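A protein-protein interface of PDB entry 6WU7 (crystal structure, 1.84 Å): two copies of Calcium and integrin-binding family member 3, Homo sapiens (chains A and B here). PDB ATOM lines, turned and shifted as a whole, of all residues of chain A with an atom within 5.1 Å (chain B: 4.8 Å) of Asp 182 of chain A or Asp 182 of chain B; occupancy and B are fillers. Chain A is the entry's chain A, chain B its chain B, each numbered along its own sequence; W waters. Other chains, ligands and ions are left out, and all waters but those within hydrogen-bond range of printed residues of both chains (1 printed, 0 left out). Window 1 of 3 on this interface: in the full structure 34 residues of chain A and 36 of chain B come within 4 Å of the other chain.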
ATOM      1  N   ARG A 108       7.313   4.705 -16.764  1.00  0.00           N
ATOM      2  CA  ARG A 108       6.933   5.466 -17.949  1.00  0.00           C
ATOM      3  C   ARG A 108       7.385   6.926 -17.850  1.00  0.00           C
ATOM      4  O   ARG A 108       7.810   7.514 -18.838  1.00  0.00           O
ATOM      5  CB  ARG A 108       5.408   5.411 -18.133  1.00  0.00           C
ATOM      6  CG  ARG A 108       4.903   5.656 -19.578  1.00  0.00           C
ATOM      7  CD  ARG A 108       3.473   5.048 -19.817  1.00  0.00           C
ATOM      8  NE  ARG A 108       2.781   5.695 -20.939  1.00  0.00           N
ATOM      9  CZ  ARG A 108       3.032   5.432 -22.225  1.00  0.00           C
ATOM     10  NH1 ARG A 108       2.356   6.081 -23.174  1.00  0.00           N
ATOM     11  NH2 ARG A 108       3.927   4.538 -22.567  1.00  0.00           N
ATOM     12  N   LEU A 139       8.334   9.056 -36.303  1.00  0.00           N
ATOM     13  CA  LEU A 139       7.428   8.087 -35.701  1.00  0.00           C
ATOM     14  C   LEU A 139       6.463   7.513 -36.734  1.00  0.00           C
ATOM     15  O   LEU A 139       6.120   6.328 -36.677  1.00  0.00           O
ATOM     16  CB  LEU A 139       6.649   8.724 -34.552  1.00  0.00           C
ATOM     17  CG  LEU A 139       7.221   8.697 -33.134  1.00  0.00           C
ATOM     18  CD1 LEU A 139       6.242   9.506 -32.257  1.00  0.00           C
ATOM     19  CD2 LEU A 139       7.428   7.310 -32.597  1.00  0.00           C
ATOM     20  N   ALA A 180      -1.628  10.151 -21.319  1.00  0.00           N
ATOM     21  CA  ALA A 180      -1.859   9.306 -22.493  1.00  0.00           C
ATOM     22  C   ALA A 180      -1.306   7.910 -22.245  1.00  0.00           C
ATOM     23  O   ALA A 180      -0.256   7.531 -22.780  1.00  0.00           O
ATOM     24  CB  ALA A 180      -1.212   9.939 -23.726  1.00  0.00           C
ATOM     25  N   PRO A 181      -1.990   7.103 -21.444  1.00  0.00           N
ATOM     26  CA  PRO A 181      -1.502   5.734 -21.200  1.00  0.00           C
ATOM     27  C   PRO A 181      -1.483   4.909 -22.481  1.00  0.00           C
ATOM     28  O   PRO A 181      -2.124   5.240 -23.476  1.00  0.00           O
ATOM     29  CB  PRO A 181      -2.505   5.153 -20.189  1.00  0.00           C
ATOM     30  CG  PRO A 181      -3.419   6.267 -19.793  1.00  0.00           C
ATOM     31  CD  PRO A 181      -3.229   7.426 -20.716  1.00  0.00           C
ATOM     32  N   ASP A 182      -0.690   3.841 -22.456  1.00  0.00           N
ATOM     33  CA  ASP A 182      -0.494   2.972 -23.625  1.00  0.00           C
ATOM     34  C   ASP A 182      -1.559   1.880 -23.588  1.00  0.00           C
ATOM     35  O   ASP A 182      -1.352   0.765 -23.113  1.00  0.00           O
ATOM     36  CB  ASP A 182       0.900   2.369 -23.644  1.00  0.00           C
ATOM     37  CG  ASP A 182       1.200   1.641 -24.928  1.00  0.00           C
ATOM     38  OD1 ASP A 182       0.272   1.402 -25.735  1.00  0.00           O
ATOM     39  OD2 ASP A 182       2.367   1.254 -25.111  1.00  0.00           O
ATOM     40  N   PHE A 183      -2.722   2.229 -24.117  1.00  0.00           N
ATOM     41  CA  PHE A 183      -3.857   1.318 -24.067  1.00  0.00           C
ATOM     42  C   PHE A 183      -3.653   0.070 -24.919  1.00  0.00           C
ATOM     43  O   PHE A 183      -4.350  -0.922 -24.691  1.00  0.00           O
ATOM     44  CB  PHE A 183      -5.122   2.022 -24.528  1.00  0.00           C
ATOM     45  CG  PHE A 183      -5.630   3.028 -23.538  1.00  0.00           C
ATOM     46  CD1 PHE A 183      -6.312   2.604 -22.418  1.00  0.00           C
ATOM     47  CD2 PHE A 183      -5.402   4.370 -23.725  1.00  0.00           C
ATOM     48  CE1 PHE A 183      -6.792   3.510 -21.491  1.00  0.00           C
ATOM     49  CE2 PHE A 183      -5.858   5.305 -22.779  1.00  0.00           C
ATOM     50  CZ  PHE A 183      -6.564   4.864 -21.675  1.00  0.00           C
ATOM     51  N   LEU A 184      -2.733   0.073 -25.885  1.00  0.00           N
ATOM     52  CA  LEU A 184      -2.550  -1.142 -26.681  1.00  0.00           C
ATOM     53  C   LEU A 184      -1.437  -2.041 -26.157  1.00  0.00           C
ATOM     54  O   LEU A 184      -1.202  -3.112 -26.738  1.00  0.00           O
ATOM     55  CB  LEU A 184      -2.280  -0.810 -28.129  1.00  0.00           C
ATOM     56  CG  LEU A 184      -3.464  -0.082 -28.781  1.00  0.00           C
ATOM     57  CD1 LEU A 184      -3.295  -0.111 -30.286  1.00  0.00           C
ATOM     58  CD2 LEU A 184      -4.799  -0.667 -28.400  1.00  0.00           C
ATOM     59  N   SER A 185      -0.763  -1.650 -25.076  1.00  0.00           N
ATOM     60  CA  SER A 185       0.351  -2.449 -24.576  1.00  0.00           C
ATOM     61  C   SER A 185      -0.093  -3.823 -24.097  1.00  0.00           C
ATOM     62  O   SER A 185       0.726  -4.744 -24.043  1.00  0.00           O
ATOM     63  CB  SER A 185       1.050  -1.700 -23.445  1.00  0.00           C
ATOM     64  OG  SER A 185       0.152  -1.430 -22.373  1.00  0.00           O
ATOM     65  N   THR A 186      -1.383  -4.010 -23.820  1.00  0.00           N
ATOM     66  CA  THR A 186      -1.817  -5.316 -23.322  1.00  0.00           C
ATOM     67  C   THR A 186      -1.686  -6.407 -24.362  1.00  0.00           C
ATOM     68  O   THR A 186      -1.516  -7.577 -24.010  1.00  0.00           O
ATOM     69  CB  THR A 186      -3.233  -5.192 -22.818  1.00  0.00           C
ATOM     70  OG1 THR A 186      -4.094  -4.735 -23.879  1.00  0.00           O
ATOM     71  CG2 THR A 186      -3.187  -4.170 -21.699  1.00  0.00           C
ATOM     72  N   LEU B 139      -2.848  -0.591 -16.044  1.00  0.00           N
ATOM     73  CA  LEU B 139      -1.796  -0.262 -16.992  1.00  0.00           C
ATOM     74  C   LEU B 139      -0.626   0.461 -16.329  1.00  0.00           C
ATOM     75  O   LEU B 139       0.508   0.354 -16.809  1.00  0.00           O
ATOM     76  CB  LEU B 139      -2.340   0.601 -18.127  1.00  0.00           C
ATOM     77  CG  LEU B 139      -3.202  -0.042 -19.207  1.00  0.00           C
ATOM     78  CD1 LEU B 139      -3.901   1.062 -19.996  1.00  0.00           C
ATOM     79  CD2 LEU B 139      -2.359  -0.906 -20.088  1.00  0.00           C
ATOM     80  N   ALA B 180      -3.344  10.191 -31.828  1.00  0.00           N
ATOM     81  CA  ALA B 180      -2.036  10.738 -31.516  1.00  0.00           C
ATOM     82  C   ALA B 180      -0.960   9.666 -31.586  1.00  0.00           C
ATOM     83  O   ALA B 180      -1.232   8.477 -31.365  1.00  0.00           O
ATOM     84  CB  ALA B 180      -2.015  11.386 -30.122  1.00  0.00           C
ATOM     85  N   PRO B 181       0.272  10.071 -31.867  1.00  0.00           N
ATOM     86  CA  PRO B 181       1.364   9.105 -31.924  1.00  0.00           C
ATOM     87  C   PRO B 181       1.683   8.608 -30.533  1.00  0.00           C
ATOM     88  O   PRO B 181       1.484   9.298 -29.534  1.00  0.00           O
ATOM     89  CB  PRO B 181       2.527   9.903 -32.524  1.00  0.00           C
ATOM     90  CG  PRO B 181       2.039  11.344 -32.640  1.00  0.00           C
ATOM     91  CD  PRO B 181       0.761  11.455 -31.876  1.00  0.00           C
ATOM     92  N   ASP B 182       2.146   7.376 -30.472  1.00  0.00           N
ATOM     93  CA  ASP B 182       2.688   6.837 -29.236  1.00  0.00           C
ATOM     94  C   ASP B 182       4.109   7.360 -29.138  1.00  0.00           C
ATOM     95  O   ASP B 182       5.024   6.828 -29.766  1.00  0.00           O
ATOM     96  CB  ASP B 182       2.635   5.319 -29.250  1.00  0.00           C
ATOM     97  CG  ASP B 182       3.206   4.715 -28.004  1.00  0.00           C
ATOM     98  OD1 ASP B 182       3.668   5.462 -27.101  1.00  0.00           O
ATOM     99  OD2 ASP B 182       3.203   3.474 -27.928  1.00  0.00           O
ATOM    100  N   PHE B 183       4.300   8.438 -28.379  1.00  0.00           N
ATOM    101  CA  PHE B 183       5.629   9.020 -28.304  1.00  0.00           C
ATOM    102  C   PHE B 183       6.623   8.119 -27.601  1.00  0.00           C
ATOM    103  O   PHE B 183       7.831   8.327 -27.746  1.00  0.00           O
ATOM    104  CB  PHE B 183       5.579  10.359 -27.592  1.00  0.00           C
ATOM    105  CG  PHE B 183       5.011  11.446 -28.434  1.00  0.00           C
ATOM    106  CD1 PHE B 183       3.667  11.768 -28.325  1.00  0.00           C
ATOM    107  CD2 PHE B 183       5.788  12.095 -29.358  1.00  0.00           C
ATOM    108  CE1 PHE B 183       3.140  12.749 -29.109  1.00  0.00           C
ATOM    109  CE2 PHE B 183       5.268  13.081 -30.141  1.00  0.00           C
ATOM    110  CZ  PHE B 183       3.936  13.401 -30.016  1.00  0.00           C
ATOM    111  N   LEU B 184       6.168   7.136 -26.839  1.00  0.00           N
ATOM    112  CA  LEU B 184       7.108   6.285 -26.115  1.00  0.00           C
ATOM    113  C   LEU B 184       7.305   4.942 -26.791  1.00  0.00           C
ATOM    114  O   LEU B 184       8.037   4.098 -26.260  1.00  0.00           O
ATOM    115  CB  LEU B 184       6.648   6.061 -24.671  1.00  0.00           C
ATOM    116  CG  LEU B 184       6.787   7.188 -23.635  1.00  0.00           C
ATOM    117  CD1 LEU B 184       6.549   6.590 -22.259  1.00  0.00           C
ATOM    118  CD2 LEU B 184       8.102   7.882 -23.721  1.00  0.00           C
ATOM    119  N   SER B 185       6.668   4.722 -27.940  1.00  0.00           N
ATOM    120  CA  SER B 185       6.782   3.419 -28.589  1.00  0.00           C
ATOM    121  C   SER B 185       8.226   3.101 -28.926  1.00  0.00           C
ATOM    122  O   SER B 185       8.624   1.931 -28.936  1.00  0.00           O
ATOM    123  CB  SER B 185       5.931   3.350 -29.869  1.00  0.00           C
ATOM    124  OG  SER B 185       6.291   4.351 -30.817  1.00  0.00           O
HETATM  125  O   HOH W   1       4.175   3.353 -25.315  1.00  0.00           O
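Among the printed residues, pairs that only touch across the chains: Arg 108 of chain A with Leu 184 of chain B (3.3 Å), Leu 139 of chain A with Pro 181 of chain B (3.7 Å), Leu 139 of chain A with Asp 182 of chain B (3.7 Å), Leu 139 of chain A with Phe 183 of chain B (3.9 Å), Leu 139 of chain A with Ser 185 of chain B (3.6 Å), Asp 182 of chain A with Leu 139 of chain B (3.6 Å), Asp 182 of chain A with Asp 182 of chain B (3.7 Å), Phe 183 of chain A with Leu 139 of chain B (3.7 Å), Ser 185 of chain A with Leu 139 of chain B (3.4 Å) and Thr 186 of chain A with Leu 139 of chain B (3.7 Å).
OD1 of Asp 182 of chain B is in hydrogen-bond range of N of Leu 184 of chain B, at 3.0 Å.
O of Ala 180 of chain A lies within hydrogen-bond range of NH1 of Arg 108 of chain A (3.0 Å).
OD1 of Asp 182 of chain A lies close to N of Leu 184 of chain A, 3.3 Å away.
The backbone carbonyl oxygen (O) of Asp 182 of chain A is in hydrogen-bond range of the side-chain hydroxyl (OG) of Ser 185 of chain A (2.8 Å).
The backbone carbonyl oxygen of Asp 182 of chain B sits at hydrogen-bond distance from the side-chain hydroxyl of Ser 185 of chain B (3.0 Å).
Printed residues of chain B that touch a printed residue of chain A: Leu 139, Pro 181, Asp 182, Phe 183, Leu 184 and Ser 185.
Hydrophobic or aromatic side chains of chain B within 4 Å of the printed part of chain A: Leu 139, Pro 181, Phe 183 and Leu 184.
Of the 9 printed residues of chain A, 6 touch a printed residue of chain B.
Hydrophobic or aromatic side chains of chain A that line the printed part of chain B: Leu 139 and Phe 183.
Among the printed residues, 10 pairs touch across the chains.
Among the printed residues, no Asp or Glu carboxylate lies within 4 Å of a Lys or Arg side-chain nitrogen of the other chain.
Water W1 lies within hydrogen-bond range of the side-chain carboxylate of Asp 182 of chain A (2.8 Å), the side-chain carboxylate of Asp 182 of chain B (2.8 Å) and the guanidinium group of Arg 108 of chain A (3.0 Å).
Leu 139 of chain A touches Pro 181 of chain B, but with the chains exchanged Pro 181 of chain A does not touch Leu 139 of chain B (4.3 Å).
Leu 139 of chain A touches Phe 183 of chain B, and with the chains exchanged Phe 183 of chain A touches Leu 139 of chain B.
Leu 139 of chain A touches Ser 185 of chain B, and with the chains exchanged Ser 185 of chain A touches Leu 139 of chain B.
Asp 182 of chain A touches its own counterpart, Asp 182 of chain B.
Positions printed for both chains: 139, 180, 181, 182, 183, 184 and 185.
Of the 10 pairs that touch across the chains among the printed residues, 7 have their exchanged pair printed and touching as well.
Asp 182 of chain A touches two residues of chain B.
Of chain A, only Leu 139 and Asp 182 come within 4 Å of Asp 182 of chain B.
Of the printed residues of chain A, Leu 139 of chain B touches Asp 182 (3.6 Å), Phe 183 (3.7 Å), Ser 185 (3.4 Å) and Thr 186 (3.7 Å).
Printed residues of chain A within 4 Å of Phe 183 of chain B: Leu 139.
Of the printed residues of chain B, Ser 185 of chain A touches Leu 139.
Of the printed residues of chain B, Arg 108 of chain A touches Leu 184.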
